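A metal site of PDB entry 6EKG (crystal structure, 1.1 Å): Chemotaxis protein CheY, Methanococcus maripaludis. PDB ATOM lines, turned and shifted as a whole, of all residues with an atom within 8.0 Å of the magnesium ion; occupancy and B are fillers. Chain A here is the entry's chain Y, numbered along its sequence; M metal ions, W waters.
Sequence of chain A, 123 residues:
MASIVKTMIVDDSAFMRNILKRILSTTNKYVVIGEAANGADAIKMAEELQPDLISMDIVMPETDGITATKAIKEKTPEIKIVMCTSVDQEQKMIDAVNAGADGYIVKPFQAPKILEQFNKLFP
Water W1 lies within hydrogen-bond range of OD1 of Asp 57 and OE1 of Gln 89.
Water W2 lies within hydrogen-bond range of the side-chain carboxylate (OD1) of Asp 11 and the side-chain amino group (NZ) of Lys 107.
The backbone NH (N) of Asp 57 is in hydrogen-bond range of the backbone carbonyl oxygen (O) of Val 10 (2.9 Å).
The side-chain carboxylate of Asp 57 is in salt-bridge range of the side-chain amino group of Lys 107, 2.9 Å away.
N of Ser 13 sits at hydrogen-bond distance from OD1 of Asp 11 (2.9 Å).
OE1 of Gln 89 is in hydrogen-bond range of N of Val 59 (2.9 Å).
OE1 of Gln 89 lies close to OD1 of Asp 57, at 3.2 Å.
The side-chain carboxylate (OD2) of Asp 11 lies within salt-bridge range of the side-chain amino group (NZ) of Lys 107.
Merely in contact with the magnesium ion: Asp 11 (3.96 Å).
Of the 18 residues printed, 4 come within 4 Å of the magnesium ion.
The nearest printed residue that does not touch the magnesium ion is Met 60 (4.1 Å).
The magnesium ion is bound by OD2 of Asp 57 (2.0 Å).
The magnesium ion is bound by water W3, at 2.0 Å.
The magnesium ion is bound by the side-chain carboxylate (OD1) of Asp 12 (2.0 Å).
The magnesium ion is bound by O of Val 59 (2.0 Å).
Water W1 is bound to the magnesium ion (2.1 Å).
Water W2 is bound to the magnesium ion (2.1 Å).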
ATOM      1  N   VAL A  10     -30.478  19.313  -5.320  1.00  0.00           N
ATOM      2  CA  VAL A  10     -29.549  18.995  -4.248  1.00  0.00           C
ATOM      3  C   VAL A  10     -28.603  17.901  -4.710  1.00  0.00           C
ATOM      4  O   VAL A  10     -29.048  16.806  -5.081  1.00  0.00           O
ATOM      5  CB  VAL A  10     -30.290  18.545  -2.976  1.00  0.00           C
ATOM      6  CG1 VAL A  10     -29.272  18.302  -1.860  1.00  0.00           C
ATOM      7  CG2 VAL A  10     -31.350  19.571  -2.578  1.00  0.00           C
ATOM      8  N   ASP A  11     -27.295  18.201  -4.709  1.00  0.00           N
ATOM      9  CA  ASP A  11     -26.290  17.208  -5.102  1.00  0.00           C
ATOM     10  C   ASP A  11     -24.941  17.775  -4.679  1.00  0.00           C
ATOM     11  O   ASP A  11     -24.707  18.964  -4.840  1.00  0.00           O
ATOM     12  CB  ASP A  11     -26.331  17.004  -6.641  1.00  0.00           C
ATOM     13  CG  ASP A  11     -25.644  15.735  -7.118  1.00  0.00           C
ATOM     14  OD1 ASP A  11     -24.530  15.462  -6.674  1.00  0.00           O
ATOM     15  OD2 ASP A  11     -26.202  15.045  -7.991  1.00  0.00           O
ATOM     16  N   ASP A  12     -24.060  16.930  -4.139  1.00  0.00           N
ATOM     17  CA  ASP A  12     -22.718  17.400  -3.797  1.00  0.00           C
ATOM     18  C   ASP A  12     -21.855  17.644  -5.030  1.00  0.00           C
ATOM     19  O   ASP A  12     -20.826  18.318  -4.925  1.00  0.00           O
ATOM     20  CB  ASP A  12     -22.040  16.478  -2.777  1.00  0.00           C
ATOM     21  CG  ASP A  12     -21.913  15.057  -3.256  1.00  0.00           C
ATOM     22  OD1 ASP A  12     -22.928  14.408  -3.563  1.00  0.00           O
ATOM     23  OD2 ASP A  12     -20.788  14.519  -3.308  1.00  0.00           O
ATOM     24  N   SER A  13     -22.249  17.156  -6.209  1.00  0.00           N
ATOM     25  CA  SER A  13     -21.494  17.357  -7.441  1.00  0.00           C
ATOM     26  C   SER A  13     -22.033  18.567  -8.204  1.00  0.00           C
ATOM     27  O   SER A  13     -23.152  18.541  -8.704  1.00  0.00           O
ATOM     28  CB  SER A  13     -21.597  16.122  -8.325  1.00  0.00           C
ATOM     29  OG  SER A  13     -21.084  16.418  -9.612  1.00  0.00           O
ATOM     30  N   MET A  16     -23.039  17.716 -11.827  1.00  0.00           N
ATOM     31  CA  MET A  16     -24.339  17.068 -11.953  1.00  0.00           C
ATOM     32  C   MET A  16     -25.475  18.058 -11.720  1.00  0.00           C
ATOM     33  O   MET A  16     -26.484  18.011 -12.415  1.00  0.00           O
ATOM     34  CB  MET A  16     -24.466  15.891 -10.979  1.00  0.00           C
ATOM     35  CG  MET A  16     -23.556  14.713 -11.283  1.00  0.00           C
ATOM     36  SD  MET A  16     -23.922  14.010 -12.922  1.00  0.00           S
ATOM     37  CE  MET A  16     -23.021  12.465 -12.831  1.00  0.00           C
ATOM     38  N   ALA A  37     -25.711  21.636  -1.723  1.00  0.00           N
ATOM     39  CA  ALA A  37     -24.633  20.662  -1.938  1.00  0.00           C
ATOM     40  C   ALA A  37     -24.532  19.619  -0.838  1.00  0.00           C
ATOM     41  O   ALA A  37     -23.650  18.768  -0.888  1.00  0.00           O
ATOM     42  CB  ALA A  37     -23.285  21.386  -2.116  1.00  0.00           C
ATOM     43  N   MET A  56     -33.176  15.150  -5.037  1.00  0.00           N
ATOM     44  CA  MET A  56     -32.339  14.906  -3.867  1.00  0.00           C
ATOM     45  C   MET A  56     -31.326  13.795  -4.150  1.00  0.00           C
ATOM     46  O   MET A  56     -31.680  12.616  -4.110  1.00  0.00           O
ATOM     47  CB  MET A  56     -33.214  14.522  -2.668  1.00  0.00           C
ATOM     48  CG  MET A  56     -32.425  14.374  -1.380  1.00  0.00           C
ATOM     49  SD  MET A  56     -32.059  15.970  -0.574  1.00  0.00           S
ATOM     50  CE  MET A  56     -33.706  16.406   0.084  1.00  0.00           C
ATOM     51  N   ASP A  57     -30.058  14.163  -4.375  1.00  0.00           N
ATOM     52  CA  ASP A  57     -28.977  13.168  -4.379  1.00  0.00           C
ATOM     53  C   ASP A  57     -29.000  12.422  -3.048  1.00  0.00           C
ATOM     54  O   ASP A  57     -29.365  12.982  -2.008  1.00  0.00           O
ATOM     55  CB  ASP A  57     -27.673  13.925  -4.570  1.00  0.00           C
ATOM     56  CG  ASP A  57     -26.477  13.015  -4.771  1.00  0.00           C
ATOM     57  OD1 ASP A  57     -26.605  11.998  -5.472  1.00  0.00           O
ATOM     58  OD2 ASP A  57     -25.363  13.373  -4.249  1.00  0.00           O
ATOM     59  N   ILE A  58     -28.619  11.157  -3.096  1.00  0.00           N
ATOM     60  CA  ILE A  58     -28.652  10.362  -1.857  1.00  0.00           C
ATOM     61  C   ILE A  58     -27.328  10.504  -1.115  1.00  0.00           C
ATOM     62  O   ILE A  58     -27.320  10.885   0.065  1.00  0.00           O
ATOM     63  CB  ILE A  58     -29.068   8.882  -2.084  1.00  0.00           C
ATOM     64  CG1 ILE A  58     -30.284   8.755  -3.026  1.00  0.00           C
ATOM     65  CG2 ILE A  58     -29.346   8.186  -0.728  1.00  0.00           C
ATOM     66  CD1 ILE A  58     -30.701   7.334  -3.380  1.00  0.00           C
ATOM     67  N   VAL A  59     -26.226  10.169  -1.764  1.00  0.00           N
ATOM     68  CA  VAL A  59     -24.925  10.129  -1.109  1.00  0.00           C
ATOM     69  C   VAL A  59     -24.280  11.518  -1.160  1.00  0.00           C
ATOM     70  O   VAL A  59     -23.895  11.993  -2.235  1.00  0.00           O
ATOM     71  CB  VAL A  59     -24.021   9.066  -1.756  1.00  0.00           C
ATOM     72  CG1 VAL A  59     -22.634   9.083  -1.129  1.00  0.00           C
ATOM     73  CG2 VAL A  59     -24.659   7.667  -1.609  1.00  0.00           C
ATOM     74  N   MET A  60     -24.178  12.139  -0.002  1.00  0.00           N
ATOM     75  CA  MET A  60     -23.554  13.448   0.138  1.00  0.00           C
ATOM     76  C   MET A  60     -22.814  13.491   1.471  1.00  0.00           C
ATOM     77  O   MET A  60     -23.264  12.907   2.407  1.00  0.00           O
ATOM     78  CB  MET A  60     -24.606  14.573   0.129  1.00  0.00           C
ATOM     79  CG  MET A  60     -25.419  14.640  -1.152  1.00  0.00           C
ATOM     80  SD  MET A  60     -26.622  16.016  -1.140  1.00  0.00           S
ATOM     81  CE  MET A  60     -27.870  15.368  -0.055  1.00  0.00           C
ATOM     82  N   PRO A  61     -21.729  14.238   1.533  1.00  0.00           N
ATOM     83  CA  PRO A  61     -20.989  14.335   2.785  1.00  0.00           C
ATOM     84  C   PRO A  61     -21.726  15.068   3.852  1.00  0.00           C
ATOM     85  O   PRO A  61     -22.556  15.899   3.584  1.00  0.00           O
ATOM     86  CB  PRO A  61     -19.746  15.126   2.438  1.00  0.00           C
ATOM     87  CG  PRO A  61     -19.922  15.641   1.087  1.00  0.00           C
ATOM     88  CD  PRO A  61     -21.178  15.097   0.486  1.00  0.00           C
ATOM     89  N   GLY A  65     -28.914  12.465   1.706  1.00  0.00           N
ATOM     90  CA  GLY A  65     -30.255  12.765   1.225  1.00  0.00           C
ATOM     91  C   GLY A  65     -31.339  11.970   1.934  1.00  0.00           C
ATOM     92  O   GLY A  65     -32.496  12.372   1.860  1.00  0.00           O
ATOM     93  N   CYS A  84     -32.223  11.413  -6.581  1.00  0.00           N
ATOM     94  CA  CYS A  84     -31.366  11.446  -7.774  1.00  0.00           C
ATOM     95  C   CYS A  84     -30.319  10.373  -7.542  1.00  0.00           C
ATOM     96  O   CYS A  84     -29.361  10.571  -6.786  1.00  0.00           O
ATOM     97  CB  CYS A  84     -30.784  12.865  -7.910  1.00  0.00           C
ATOM     98  SG  CYS A  84     -29.928  13.084  -9.418  1.00  0.00           S
ATOM     99  N   SER A  86     -28.094   6.612  -8.802  1.00  0.00           N
ATOM    100  CA  SER A  86     -27.092   6.152  -9.773  1.00  0.00           C
ATOM    101  C   SER A  86     -26.614   4.800  -9.274  1.00  0.00           C
ATOM    102  O   SER A  86     -26.899   4.422  -8.139  1.00  0.00           O
ATOM    103  CB  SER A  86     -25.927   7.132  -9.916  1.00  0.00           C
ATOM    104  OG  SER A  86     -25.383   7.418  -8.646  1.00  0.00           O
ATOM    105  N   ASP A  88     -23.810   3.741  -8.203  1.00  0.00           N
ATOM    106  CA  ASP A  88     -23.020   3.808  -6.969  1.00  0.00           C
ATOM    107  C   ASP A  88     -23.842   4.150  -5.738  1.00  0.00           C
ATOM    108  O   ASP A  88     -23.298   4.066  -4.636  1.00  0.00           O
ATOM    109  CB  ASP A  88     -21.920   4.839  -7.137  1.00  0.00           C
ATOM    110  CG  ASP A  88     -22.475   6.171  -7.448  1.00  0.00           C
ATOM    111  OD1 ASP A  88     -22.482   7.028  -6.552  1.00  0.00           O
ATOM    112  OD2 ASP A  88     -22.960   6.347  -8.584  1.00  0.00           O
ATOM    113  N   GLN A  89     -25.113   4.498  -5.880  1.00  0.00           N
ATOM    114  CA  GLN A  89     -26.007   4.782  -4.751  1.00  0.00           C
ATOM    115  C   GLN A  89     -27.057   3.701  -4.551  1.00  0.00           C
ATOM    116  O   GLN A  89     -27.920   3.856  -3.686  1.00  0.00           O
ATOM    117  CB  GLN A  89     -26.696   6.133  -4.952  1.00  0.00           C
ATOM    118  CG  GLN A  89     -25.724   7.293  -5.204  1.00  0.00           C
ATOM    119  CD  GLN A  89     -26.488   8.562  -5.324  1.00  0.00           C
ATOM    120  OE1 GLN A  89     -26.976   9.088  -4.322  1.00  0.00           O
ATOM    121  NE2 GLN A  89     -26.708   9.031  -6.537  1.00  0.00           N
ATOM    122  N   LYS A 107     -28.919   9.388 -12.593  1.00  0.00           N
ATOM    123  CA  LYS A 107     -27.686   9.820 -13.239  1.00  0.00           C
ATOM    124  C   LYS A 107     -27.005   8.567 -13.796  1.00  0.00           C
ATOM    125  O   LYS A 107     -26.963   7.536 -13.095  1.00  0.00           O
ATOM    126  CB  LYS A 107     -26.755  10.445 -12.223  1.00  0.00           C
ATOM    127  CG  LYS A 107     -27.281  11.728 -11.643  1.00  0.00           C
ATOM    128  CD  LYS A 107     -26.404  12.352 -10.529  1.00  0.00           C
ATOM    129  CE  LYS A 107     -26.476  11.608  -9.194  1.00  0.00           C
ATOM    130  NZ  LYS A 107     -25.610  12.319  -8.173  1.00  0.00           N
HETATM  131 MG    MG M   1     -23.537  12.569  -4.159  1.00  0.00          MG
HETATM  132  O   HOH W   1     -24.229  10.753  -4.842  1.00  0.00           O
HETATM  133  O   HOH W   2     -23.232  13.156  -6.138  1.00  0.00           O
HETATM  134  O   HOH W   3     -21.666  11.887  -3.983  1.00  0.00           O
